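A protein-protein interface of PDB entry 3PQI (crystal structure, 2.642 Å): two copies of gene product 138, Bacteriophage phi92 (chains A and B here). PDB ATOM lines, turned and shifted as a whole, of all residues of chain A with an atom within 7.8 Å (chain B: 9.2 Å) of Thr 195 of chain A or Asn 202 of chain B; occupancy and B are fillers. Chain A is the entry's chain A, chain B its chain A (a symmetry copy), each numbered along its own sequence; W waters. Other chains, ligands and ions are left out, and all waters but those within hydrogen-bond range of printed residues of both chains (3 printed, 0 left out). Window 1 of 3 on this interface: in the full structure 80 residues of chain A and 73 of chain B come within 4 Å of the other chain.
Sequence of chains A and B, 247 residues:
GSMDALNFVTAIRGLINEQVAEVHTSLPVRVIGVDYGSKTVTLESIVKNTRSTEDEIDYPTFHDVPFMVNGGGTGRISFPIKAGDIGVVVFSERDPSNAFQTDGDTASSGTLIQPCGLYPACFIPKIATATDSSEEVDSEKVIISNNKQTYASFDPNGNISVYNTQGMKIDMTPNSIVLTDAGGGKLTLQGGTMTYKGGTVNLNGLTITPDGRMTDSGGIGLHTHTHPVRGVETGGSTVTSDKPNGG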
ATOM      1  N   ILE A 177     -10.329 -26.219  24.311  1.00  0.00           N
ATOM      2  CA  ILE A 177      -9.839 -27.519  23.895  1.00  0.00           C
ATOM      3  C   ILE A 177      -9.192 -27.325  22.532  1.00  0.00           C
ATOM      4  O   ILE A 177      -9.802 -26.764  21.619  1.00  0.00           O
ATOM      5  CB  ILE A 177     -10.976 -28.550  23.775  1.00  0.00           C
ATOM      6  CG1 ILE A 177     -11.536 -28.904  25.158  1.00  0.00           C
ATOM      7  CG2 ILE A 177     -10.484 -29.808  23.046  1.00  0.00           C
ATOM      8  CD1 ILE A 177     -12.686 -29.888  25.117  1.00  0.00           C
ATOM      9  N   VAL A 178      -7.956 -27.778  22.392  1.00  0.00           N
ATOM     10  CA  VAL A 178      -7.225 -27.564  21.154  1.00  0.00           C
ATOM     11  C   VAL A 178      -6.595 -28.855  20.684  1.00  0.00           C
ATOM     12  O   VAL A 178      -5.981 -29.578  21.468  1.00  0.00           O
ATOM     13  CB  VAL A 178      -6.113 -26.491  21.320  1.00  0.00           C
ATOM     14  CG1 VAL A 178      -5.354 -26.308  20.020  1.00  0.00           C
ATOM     15  CG2 VAL A 178      -6.705 -25.165  21.790  1.00  0.00           C
ATOM     16  N   LEU A 179      -6.765 -29.145  19.399  1.00  0.00           N
ATOM     17  CA  LEU A 179      -6.117 -30.291  18.773  1.00  0.00           C
ATOM     18  C   LEU A 179      -5.041 -29.786  17.824  1.00  0.00           C
ATOM     19  O   LEU A 179      -5.322 -29.005  16.911  1.00  0.00           O
ATOM     20  CB  LEU A 179      -7.136 -31.132  18.005  1.00  0.00           C
ATOM     21  CG  LEU A 179      -7.971 -32.126  18.813  1.00  0.00           C
ATOM     22  CD1 LEU A 179      -8.496 -31.498  20.090  1.00  0.00           C
ATOM     23  CD2 LEU A 179      -9.114 -32.660  17.962  1.00  0.00           C
ATOM     24  N   LYS A 186      -4.748 -27.035  12.971  1.00  0.00           N
ATOM     25  CA  LYS A 186      -5.139 -26.808  14.353  1.00  0.00           C
ATOM     26  C   LYS A 186      -6.656 -26.681  14.489  1.00  0.00           C
ATOM     27  O   LYS A 186      -7.283 -25.851  13.827  1.00  0.00           O
ATOM     28  CB  LYS A 186      -4.423 -25.574  14.916  1.00  0.00           C
ATOM     29  CG  LYS A 186      -4.656 -25.352  16.403  1.00  0.00           C
ATOM     30  CD  LYS A 186      -3.651 -24.381  17.006  1.00  0.00           C
ATOM     31  CE  LYS A 186      -2.253 -24.989  17.058  1.00  0.00           C
ATOM     32  NZ  LYS A 186      -1.304 -24.161  17.866  1.00  0.00           N
ATOM     33  N   LEU A 187      -7.238 -27.524  15.338  1.00  0.00           N
ATOM     34  CA  LEU A 187      -8.666 -27.450  15.641  1.00  0.00           C
ATOM     35  C   LEU A 187      -8.865 -26.877  17.047  1.00  0.00           C
ATOM     36  O   LEU A 187      -8.230 -27.324  18.003  1.00  0.00           O
ATOM     37  CB  LEU A 187      -9.322 -28.832  15.521  1.00  0.00           C
ATOM     38  CG  LEU A 187     -10.831 -28.891  15.802  1.00  0.00           C
ATOM     39  CD1 LEU A 187     -11.635 -28.261  14.662  1.00  0.00           C
ATOM     40  CD2 LEU A 187     -11.303 -30.317  16.064  1.00  0.00           C
ATOM     41  N   THR A 188      -9.743 -25.886  17.172  1.00  0.00           N
ATOM     42  CA  THR A 188      -9.893 -25.165  18.434  1.00  0.00           C
ATOM     43  C   THR A 188     -11.345 -24.972  18.849  1.00  0.00           C
ATOM     44  O   THR A 188     -12.171 -24.495  18.068  1.00  0.00           O
ATOM     45  CB  THR A 188      -9.229 -23.769  18.369  1.00  0.00           C
ATOM     46  OG1 THR A 188      -7.817 -23.909  18.163  1.00  0.00           O
ATOM     47  CG2 THR A 188      -9.485 -22.989  19.654  1.00  0.00           C
ATOM     48  N   LEU A 189     -11.646 -25.347  20.089  1.00  0.00           N
ATOM     49  CA  LEU A 189     -12.945 -25.057  20.690  1.00  0.00           C
ATOM     50  C   LEU A 189     -12.741 -24.107  21.858  1.00  0.00           C
ATOM     51  O   LEU A 189     -12.102 -24.457  22.851  1.00  0.00           O
ATOM     52  CB  LEU A 189     -13.643 -26.332  21.173  1.00  0.00           C
ATOM     53  CG  LEU A 189     -14.328 -27.203  20.116  1.00  0.00           C
ATOM     54  CD1 LEU A 189     -13.305 -27.993  19.309  1.00  0.00           C
ATOM     55  CD2 LEU A 189     -15.323 -28.138  20.781  1.00  0.00           C
ATOM     56  N   GLN A 190     -13.283 -22.902  21.734  1.00  0.00           N
ATOM     57  CA  GLN A 190     -13.061 -21.867  22.728  1.00  0.00           C
ATOM     58  C   GLN A 190     -14.096 -20.763  22.582  1.00  0.00           C
ATOM     59  O   GLN A 190     -14.496 -20.419  21.465  1.00  0.00           O
ATOM     60  CB  GLN A 190     -11.657 -21.286  22.567  1.00  0.00           C
ATOM     61  CG  GLN A 190     -11.258 -20.297  23.644  1.00  0.00           C
ATOM     62  CD  GLN A 190      -9.820 -19.833  23.505  1.00  0.00           C
ATOM     63  OE1 GLN A 190      -9.312 -19.674  22.396  1.00  0.00           O
ATOM     64  NE2 GLN A 190      -9.152 -19.623  24.635  1.00  0.00           N
ATOM     65  N   THR A 193     -17.093 -21.174  20.386  1.00  0.00           N
ATOM     66  CA  THR A 193     -16.887 -21.163  18.944  1.00  0.00           C
ATOM     67  C   THR A 193     -15.944 -22.288  18.558  1.00  0.00           C
ATOM     68  O   THR A 193     -15.104 -22.706  19.354  1.00  0.00           O
ATOM     69  CB  THR A 193     -16.267 -19.838  18.459  1.00  0.00           C
ATOM     70  OG1 THR A 193     -14.850 -19.855  18.690  1.00  0.00           O
ATOM     71  CG2 THR A 193     -16.884 -18.654  19.189  1.00  0.00           C
ATOM     72  N   MET A 194     -16.078 -22.780  17.334  1.00  0.00           N
ATOM     73  CA  MET A 194     -15.161 -23.800  16.850  1.00  0.00           C
ATOM     74  C   MET A 194     -14.427 -23.336  15.605  1.00  0.00           C
ATOM     75  O   MET A 194     -15.021 -22.747  14.700  1.00  0.00           O
ATOM     76  CB  MET A 194     -15.884 -25.118  16.577  1.00  0.00           C
ATOM     77  CG  MET A 194     -14.923 -26.272  16.355  1.00  0.00           C
ATOM     78  SD  MET A 194     -15.724 -27.863  16.086  1.00  0.00           S
ATOM     79  CE  MET A 194     -16.588 -27.530  14.547  1.00  0.00           C
ATOM     80  N   THR A 195     -13.131 -23.616  15.560  1.00  0.00           N
ATOM     81  CA  THR A 195     -12.295 -23.148  14.468  1.00  0.00           C
ATOM     82  C   THR A 195     -11.325 -24.224  13.991  1.00  0.00           C
ATOM     83  O   THR A 195     -10.730 -24.941  14.794  1.00  0.00           O
ATOM     84  CB  THR A 195     -11.483 -21.901  14.891  1.00  0.00           C
ATOM     85  OG1 THR A 195     -12.379 -20.858  15.300  1.00  0.00           O
ATOM     86  CG2 THR A 195     -10.618 -21.410  13.741  1.00  0.00           C
ATOM     87  N   TYR A 196     -11.180 -24.344  12.678  1.00  0.00           N
ATOM     88  CA  TYR A 196     -10.076 -25.109  12.127  1.00  0.00           C
ATOM     89  C   TYR A 196      -9.261 -24.229  11.205  1.00  0.00           C
ATOM     90  O   TYR A 196      -9.795 -23.632  10.270  1.00  0.00           O
ATOM     91  CB  TYR A 196     -10.539 -26.350  11.363  1.00  0.00           C
ATOM     92  CG  TYR A 196      -9.376 -27.080  10.722  1.00  0.00           C
ATOM     93  CD1 TYR A 196      -8.588 -27.954  11.461  1.00  0.00           C
ATOM     94  CD2 TYR A 196      -9.041 -26.868   9.390  1.00  0.00           C
ATOM     95  CE1 TYR A 196      -7.513 -28.607  10.892  1.00  0.00           C
ATOM     96  CE2 TYR A 196      -7.963 -27.523   8.809  1.00  0.00           C
ATOM     97  CZ  TYR A 196      -7.202 -28.395   9.569  1.00  0.00           C
ATOM     98  OH  TYR A 196      -6.123 -29.063   9.024  1.00  0.00           O
ATOM     99  N   LYS A 197      -7.968 -24.145  11.487  1.00  0.00           N
ATOM    100  CA  LYS A 197      -7.030 -23.497  10.585  1.00  0.00           C
ATOM    101  C   LYS A 197      -5.959 -24.486  10.152  1.00  0.00           C
ATOM    102  O   LYS A 197      -5.249 -25.058  10.983  1.00  0.00           O
ATOM    103  CB  LYS A 197      -6.382 -22.278  11.239  1.00  0.00           C
ATOM    104  CG  LYS A 197      -5.313 -21.642  10.364  1.00  0.00           C
ATOM    105  CD  LYS A 197      -5.376 -20.127  10.405  1.00  0.00           C
ATOM    106  CE  LYS A 197      -4.726 -19.520   9.169  1.00  0.00           C
ATOM    107  NZ  LYS A 197      -5.403 -19.967   7.917  1.00  0.00           N
ATOM    108  N   GLY A 198      -5.850 -24.686   8.845  1.00  0.00           N
ATOM    109  CA  GLY A 198      -4.857 -25.580   8.283  1.00  0.00           C
ATOM    110  C   GLY A 198      -5.102 -25.774   6.803  1.00  0.00           C
ATOM    111  O   GLY A 198      -5.424 -24.821   6.086  1.00  0.00           O
ATOM    112  N   VAL A 201     -10.068 -29.164   4.181  1.00  0.00           N
ATOM    113  CA  VAL A 201     -11.051 -29.848   5.008  1.00  0.00           C
ATOM    114  C   VAL A 201     -11.922 -30.743   4.123  1.00  0.00           C
ATOM    115  O   VAL A 201     -12.360 -30.325   3.049  1.00  0.00           O
ATOM    116  CB  VAL A 201     -11.939 -28.828   5.752  1.00  0.00           C
ATOM    117  CG1 VAL A 201     -13.032 -29.533   6.543  1.00  0.00           C
ATOM    118  CG2 VAL A 201     -11.084 -27.952   6.657  1.00  0.00           C
ATOM    119  N   ILE A 208     -13.303 -28.000   1.485  1.00  0.00           N
ATOM    120  CA  ILE A 208     -13.011 -26.599   1.742  1.00  0.00           C
ATOM    121  C   ILE A 208     -11.503 -26.368   1.664  1.00  0.00           C
ATOM    122  O   ILE A 208     -10.733 -26.982   2.402  1.00  0.00           O
ATOM    123  CB  ILE A 208     -13.537 -26.168   3.120  1.00  0.00           C
ATOM    124  CG1 ILE A 208     -14.997 -26.592   3.272  1.00  0.00           C
ATOM    125  CG2 ILE A 208     -13.367 -24.664   3.313  1.00  0.00           C
ATOM    126  CD1 ILE A 208     -15.584 -26.303   4.622  1.00  0.00           C
ATOM    127  N   GLY A 212     -10.400 -21.200   2.308  1.00  0.00           N
ATOM    128  CA  GLY A 212     -11.793 -21.063   2.697  1.00  0.00           C
ATOM    129  C   GLY A 212     -12.830 -21.038   1.588  1.00  0.00           C
ATOM    130  O   GLY A 212     -13.895 -20.438   1.746  1.00  0.00           O
ATOM    131  N   ASP B 181     -17.363 -27.587  25.369  1.00  0.00           N
ATOM    132  CA  ASP B 181     -16.831 -26.254  25.603  1.00  0.00           C
ATOM    133  C   ASP B 181     -17.752 -25.478  26.545  1.00  0.00           C
ATOM    134  O   ASP B 181     -18.797 -24.967  26.132  1.00  0.00           O
ATOM    135  CB  ASP B 181     -16.648 -25.512  24.275  1.00  0.00           C
ATOM    136  CG  ASP B 181     -16.175 -24.082  24.462  1.00  0.00           C
ATOM    137  OD1 ASP B 181     -15.810 -23.717  25.601  1.00  0.00           O
ATOM    138  OD2 ASP B 181     -16.161 -23.324  23.467  1.00  0.00           O
ATOM    139  N   LEU B 187     -19.226 -30.484  20.618  1.00  0.00           N
ATOM    140  CA  LEU B 187     -18.971 -31.324  19.450  1.00  0.00           C
ATOM    141  C   LEU B 187     -19.267 -32.787  19.793  1.00  0.00           C
ATOM    142  O   LEU B 187     -18.807 -33.297  20.817  1.00  0.00           O
ATOM    143  CB  LEU B 187     -17.525 -31.162  18.966  1.00  0.00           C
ATOM    144  CG  LEU B 187     -17.129 -31.985  17.730  1.00  0.00           C
ATOM    145  CD1 LEU B 187     -17.760 -31.417  16.457  1.00  0.00           C
ATOM    146  CD2 LEU B 187     -15.614 -32.084  17.577  1.00  0.00           C
ATOM    147  N   TYR B 196     -21.952 -30.340  15.591  1.00  0.00           N
ATOM    148  CA  TYR B 196     -21.514 -29.248  16.443  1.00  0.00           C
ATOM    149  C   TYR B 196     -22.668 -28.304  16.691  1.00  0.00           C
ATOM    150  O   TYR B 196     -23.290 -27.807  15.751  1.00  0.00           O
ATOM    151  CB  TYR B 196     -20.341 -28.467  15.847  1.00  0.00           C
ATOM    152  CG  TYR B 196     -19.962 -27.281  16.711  1.00  0.00           C
ATOM    153  CD1 TYR B 196     -19.154 -27.442  17.829  1.00  0.00           C
ATOM    154  CD2 TYR B 196     -20.442 -26.006  16.432  1.00  0.00           C
ATOM    155  CE1 TYR B 196     -18.821 -26.372  18.634  1.00  0.00           C
ATOM    156  CE2 TYR B 196     -20.109 -24.923  17.234  1.00  0.00           C
ATOM    157  CZ  TYR B 196     -19.295 -25.115  18.337  1.00  0.00           C
ATOM    158  OH  TYR B 196     -18.944 -24.060  19.157  1.00  0.00           O
ATOM    159  N   GLY B 199     -21.576 -21.671  18.849  1.00  0.00           N
ATOM    160  CA  GLY B 199     -21.456 -20.414  18.135  1.00  0.00           C
ATOM    161  C   GLY B 199     -20.830 -20.564  16.763  1.00  0.00           C
ATOM    162  O   GLY B 199     -20.832 -21.648  16.176  1.00  0.00           O
ATOM    163  N   THR B 200     -20.284 -19.463  16.256  1.00  0.00           N
ATOM    164  CA  THR B 200     -19.710 -19.416  14.916  1.00  0.00           C
ATOM    165  C   THR B 200     -18.654 -20.488  14.676  1.00  0.00           C
ATOM    166  O   THR B 200     -17.700 -20.631  15.447  1.00  0.00           O
ATOM    167  CB  THR B 200     -19.072 -18.043  14.625  1.00  0.00           C
ATOM    168  OG1 THR B 200     -20.093 -17.039  14.578  1.00  0.00           O
ATOM    169  CG2 THR B 200     -18.331 -18.071  13.297  1.00  0.00           C
ATOM    170  N   VAL B 201     -18.835 -21.231  13.588  1.00  0.00           N
ATOM    171  CA  VAL B 201     -17.852 -22.199  13.126  1.00  0.00           C
ATOM    172  C   VAL B 201     -16.954 -21.546  12.074  1.00  0.00           C
ATOM    173  O   VAL B 201     -17.442 -20.846  11.182  1.00  0.00           O
ATOM    174  CB  VAL B 201     -18.550 -23.437  12.522  1.00  0.00           C
ATOM    175  CG1 VAL B 201     -17.529 -24.410  11.948  1.00  0.00           C
ATOM    176  CG2 VAL B 201     -19.423 -24.110  13.571  1.00  0.00           C
ATOM    177  N   ASN B 202     -15.647 -21.768  12.182  1.00  0.00           N
ATOM    178  CA  ASN B 202     -14.684 -21.176  11.255  1.00  0.00           C
ATOM    179  C   ASN B 202     -13.774 -22.235  10.652  1.00  0.00           C
ATOM    180  O   ASN B 202     -12.990 -22.866  11.362  1.00  0.00           O
ATOM    181  CB  ASN B 202     -13.845 -20.119  11.975  1.00  0.00           C
ATOM    182  CG  ASN B 202     -12.951 -19.326  11.031  1.00  0.00           C
ATOM    183  OD1 ASN B 202     -12.225 -19.885  10.204  1.00  0.00           O
ATOM    184  ND2 ASN B 202     -13.003 -18.007  11.156  1.00  0.00           N
ATOM    185  N   LEU B 203     -13.881 -22.430   9.342  1.00  0.00           N
ATOM    186  CA  LEU B 203     -13.027 -23.384   8.642  1.00  0.00           C
ATOM    187  C   LEU B 203     -12.207 -22.678   7.570  1.00  0.00           C
ATOM    188  O   LEU B 203     -12.700 -22.423   6.472  1.00  0.00           O
ATOM    189  CB  LEU B 203     -13.869 -24.489   8.004  1.00  0.00           C
ATOM    190  CG  LEU B 203     -14.891 -25.133   8.947  1.00  0.00           C
ATOM    191  CD1 LEU B 203     -15.840 -26.072   8.201  1.00  0.00           C
ATOM    192  CD2 LEU B 203     -14.197 -25.853  10.102  1.00  0.00           C
ATOM    193  N   ASN B 204     -10.960 -22.354   7.899  1.00  0.00           N
ATOM    194  CA  ASN B 204     -10.068 -21.668   6.965  1.00  0.00           C
ATOM    195  C   ASN B 204     -10.695 -20.421   6.345  1.00  0.00           C
ATOM    196  O   ASN B 204     -10.562 -20.185   5.147  1.00  0.00           O
ATOM    197  CB  ASN B 204      -9.619 -22.613   5.849  1.00  0.00           C
ATOM    198  CG  ASN B 204      -8.827 -23.800   6.367  1.00  0.00           C
ATOM    199  OD1 ASN B 204      -8.194 -23.731   7.422  1.00  0.00           O
ATOM    200  ND2 ASN B 204      -8.853 -24.894   5.620  1.00  0.00           N
ATOM    201  N   GLY B 205     -11.379 -19.627   7.161  1.00  0.00           N
ATOM    202  CA  GLY B 205     -12.010 -18.412   6.679  1.00  0.00           C
ATOM    203  C   GLY B 205     -13.497 -18.570   6.417  1.00  0.00           C
ATOM    204  O   GLY B 205     -14.277 -17.650   6.659  1.00  0.00           O
ATOM    205  N   LEU B 206     -13.888 -19.734   5.911  1.00  0.00           N
ATOM    206  CA  LEU B 206     -15.295 -20.016   5.664  1.00  0.00           C
ATOM    207  C   LEU B 206     -16.048 -20.035   6.994  1.00  0.00           C
ATOM    208  O   LEU B 206     -15.586 -20.637   7.964  1.00  0.00           O
ATOM    209  CB  LEU B 206     -15.443 -21.347   4.923  1.00  0.00           C
ATOM    210  CG  LEU B 206     -16.850 -21.757   4.477  1.00  0.00           C
ATOM    211  CD1 LEU B 206     -16.783 -22.698   3.283  1.00  0.00           C
ATOM    212  CD2 LEU B 206     -17.630 -22.387   5.626  1.00  0.00           C
ATOM    213  N   THR B 207     -17.200 -19.370   7.043  1.00  0.00           N
ATOM    214  CA  THR B 207     -17.922 -19.208   8.307  1.00  0.00           C
ATOM    215  C   THR B 207     -19.362 -19.719   8.301  1.00  0.00           C
ATOM    216  O   THR B 207     -20.097 -19.556   7.327  1.00  0.00           O
ATOM    217  CB  THR B 207     -17.935 -17.732   8.784  1.00  0.00           C
ATOM    218  OG1 THR B 207     -18.457 -16.891   7.747  1.00  0.00           O
ATOM    219  CG2 THR B 207     -16.536 -17.273   9.160  1.00  0.00           C
ATOM    220  N   ILE B 208     -19.753 -20.331   9.414  1.00  0.00           N
ATOM    221  CA  ILE B 208     -21.127 -20.761   9.624  1.00  0.00           C
ATOM    222  C   ILE B 208     -21.658 -20.159  10.924  1.00  0.00           C
ATOM    223  O   ILE B 208     -21.097 -20.383  11.997  1.00  0.00           O
ATOM    224  CB  ILE B 208     -21.225 -22.293   9.677  1.00  0.00           C
ATOM    225  CG1 ILE B 208     -20.505 -22.900   8.473  1.00  0.00           C
ATOM    226  CG2 ILE B 208     -22.684 -22.736   9.740  1.00  0.00           C
ATOM    227  CD1 ILE B 208     -20.459 -24.399   8.477  1.00  0.00           C
ATOM    228  N   THR B 209     -22.732 -19.384  10.819  1.00  0.00           N
ATOM    229  CA  THR B 209     -23.306 -18.703  11.975  1.00  0.00           C
ATOM    230  C   THR B 209     -23.869 -19.690  12.997  1.00  0.00           C
ATOM    231  O   THR B 209     -24.018 -20.877  12.702  1.00  0.00           O
ATOM    232  CB  THR B 209     -24.415 -17.708  11.550  1.00  0.00           C
ATOM    233  OG1 THR B 209     -25.408 -18.388  10.769  1.00  0.00           O
ATOM    234  CG2 THR B 209     -23.824 -16.567  10.733  1.00  0.00           C
ATOM    235  N   PRO B 210     -24.175 -19.202  14.209  1.00  0.00           N
ATOM    236  CA  PRO B 210     -24.817 -20.031  15.236  1.00  0.00           C
ATOM    237  C   PRO B 210     -26.167 -20.568  14.771  1.00  0.00           C
ATOM    238  O   PRO B 210     -26.641 -21.578  15.286  1.00  0.00           O
ATOM    239  CB  PRO B 210     -25.017 -19.053  16.394  1.00  0.00           C
ATOM    240  CG  PRO B 210     -23.956 -18.027  16.201  1.00  0.00           C
ATOM    241  CD  PRO B 210     -23.816 -17.868  14.721  1.00  0.00           C
ATOM    242  N   THR B 215     -21.018 -18.619   4.807  1.00  0.00           N
ATOM    243  CA  THR B 215     -20.422 -17.665   3.890  1.00  0.00           C
ATOM    244  C   THR B 215     -18.953 -18.034   3.748  1.00  0.00           C
ATOM    245  O   THR B 215     -18.252 -18.185   4.750  1.00  0.00           O
ATOM    246  CB  THR B 215     -20.509 -16.237   4.461  1.00  0.00           C
ATOM    247  OG1 THR B 215     -21.875 -15.910   4.750  1.00  0.00           O
ATOM    248  CG2 THR B 215     -19.947 -15.230   3.480  1.00  0.00           C
ATOM    249  N   ASP B 216     -18.478 -18.194   2.517  1.00  0.00           N
ATOM    250  CA  ASP B 216     -17.081 -18.563   2.319  1.00  0.00           C
ATOM    251  C   ASP B 216     -16.164 -17.406   2.697  1.00  0.00           C
ATOM    252  O   ASP B 216     -16.629 -16.322   3.055  1.00  0.00           O
ATOM    253  CB  ASP B 216     -16.814 -19.040   0.883  1.00  0.00           C
ATOM    254  CG  ASP B 216     -16.959 -17.928  -0.151  1.00  0.00           C
ATOM    255  OD1 ASP B 216     -17.018 -16.744   0.229  1.00  0.00           O
ATOM    256  OD2 ASP B 216     -16.998 -18.238  -1.358  1.00  0.00           O
ATOM    257  N   SER B 217     -14.860 -17.648   2.623  1.00  0.00           N
ATOM    258  CA  SER B 217     -13.870 -16.635   2.968  1.00  0.00           C
ATOM    259  C   SER B 217     -14.005 -15.374   2.116  1.00  0.00           C
ATOM    260  O   SER B 217     -13.652 -14.280   2.557  1.00  0.00           O
ATOM    261  CB  SER B 217     -12.462 -17.212   2.823  1.00  0.00           C
ATOM    262  OG  SER B 217     -12.268 -17.745   1.524  1.00  0.00           O
HETATM  263  O   HOH W   1      -5.486 -22.285   6.028  1.00  0.00           O
HETATM  264  O   HOH W   2     -17.284 -24.492  21.107  1.00  0.00           O
HETATM  265  O   HOH W   3     -15.162 -18.843  14.939  1.00  0.00           O
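The side-chain carboxylate of Asp 181 of chain B is in hydrogen-bond range of the backbone NH of Gln 190 of chain A, at 3.4 Å.
The backbone NH of Met 194 of chain A lies within hydrogen-bond range of the backbone carbonyl oxygen of Thr 200 of chain B, 3.3 Å away.
N of Asn 202 of chain B sits at hydrogen-bond distance from O of Met 194 of chain A, at 2.8 Å.
The backbone NH of Tyr 196 of chain A sits at hydrogen-bond distance from the backbone carbonyl oxygen of Asn 202 of chain B (2.7 Å).
The backbone NH of Asn 204 of chain B lies within hydrogen-bond range of the backbone carbonyl oxygen of Tyr 196 of chain A, at 2.9 Å.
The side-chain amide oxygen (OD1) of Asn 204 of chain B lies within hydrogen-bond range of the backbone NH (N) of Gly 198 of chain A, at 2.9 Å.
N of Gly 212 of chain A sits close to O of Asn 204 of chain B, 3.0 Å away.
The backbone carbonyl oxygen (O) of Gly 212 of chain A is in hydrogen-bond range of the backbone NH (N) of Ser 217 of chain B, 3.1 Å away.
The backbone carbonyl oxygen (O) of Ile 177 of chain A is in hydrogen-bond range of the backbone NH (N) of Leu 189 of chain A, at 2.8 Å.
The backbone carbonyl oxygen (O) of Lys 197 of chain A is in hydrogen-bond range of the backbone NH (N) of Lys 186 of chain A (2.8 Å).
The backbone carbonyl oxygen (O) of Thr 195 of chain A lies within hydrogen-bond range of the backbone NH (N) of Thr 188 of chain A (2.7 Å).
The backbone carbonyl oxygen (O) of Ile 208 of chain A lies within hydrogen-bond range of the backbone NH (N) of Val 201 of chain A.
N of Val 201 of chain B sits at hydrogen-bond distance from O of Ile 208 of chain B (2.9 Å).
The side-chain amide oxygen of Asn 202 of chain B sits at hydrogen-bond distance from the backbone NH of Gly 205 of chain B (3.2 Å).
Among the printed residues, pairs that only touch across the chains: Thr 195 of chain A with Asn 202 of chain B, Met 194 of chain A with Val 201 of chain B, Gly 212 of chain A with Asp 216 of chain B, Lys 197 of chain A with Asn 204 of chain B, Thr 193 of chain A with Thr 200 of chain B, Thr 193 of chain A with Tyr 196 of chain B, Ile 208 of chain A with Leu 203 of chain B, Tyr 196 of chain A with Leu 203 of chain B, Met 194 of chain A with Tyr 196 of chain B, Gly 212 of chain A with Leu 206 of chain B, Leu 189 of chain A with Asp 181 of chain B, Thr 193 of chain A with Asp 181 of chain B, Val 201 of chain A with Asn 204 of chain B and Ile 208 of chain A with Leu 206 of chain B.
Val 178 of chain A touches none of the printed residues of chain B.
Printed residues of chain B within 4 Å of Thr 193 of chain A: Asp 181 (3.9 Å), Tyr 196 (3.5 Å) and Thr 200 (3.4 Å).
Of the printed residues of chain B, Thr 195 of chain A touches Asn 202.
Printed residues of chain B within 4 Å of Gly 198 of chain A: Asn 204.
Of the printed residues of chain B, Val 201 of chain A touches Asn 204.
Printed residues of chain B within 4 Å of Ile 208 of chain A: Leu 203 and Leu 206.
Of the printed residues of chain A, Val 201 of chain B touches Met 194 (3.3 Å).
The nearest residue of chain B that does not touch Thr 195 of chain A is Leu 203 of chain B (5.1 Å).
The nearest residue of chain A that does not touch Asn 202 of chain B is Lys 197 of chain A (5.2 Å).
Along chain A the printed residues that touch a printed residue of chain B span positions 189 to 212.
Hydrophobic or aromatic side chains of chain B that line the printed part of chain A: Tyr 196, Leu 203 and Leu 206.
Among the printed residues, 22 pairs touch across the chains.
Among the printed residues, no Asp or Glu carboxylate lies within 4 Å of a Lys or Arg side-chain nitrogen of the other chain.
4 positions are printed for both chains.
Of the 22 pairs that touch across the chains among the printed residues, none has its exchanged pair printed and touching as well.
Water W1 lies within hydrogen-bond range of O of Gly 198 of chain A (2.5 Å), NZ of Lys 197 of chain A (3.0 Å) and OD1 of Asn 204 of chain B (3.4 Å).
Water W2 lies within hydrogen-bond range of OH of Tyr 196 of chain B (2.6 Å), OD2 of Asp 181 of chain B (2.9 Å) and O of Thr 193 of chain A (3.3 Å).
Water W3 lies within hydrogen-bond range of O of Thr 200 of chain B and OG1 of Thr 195 of chain A.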
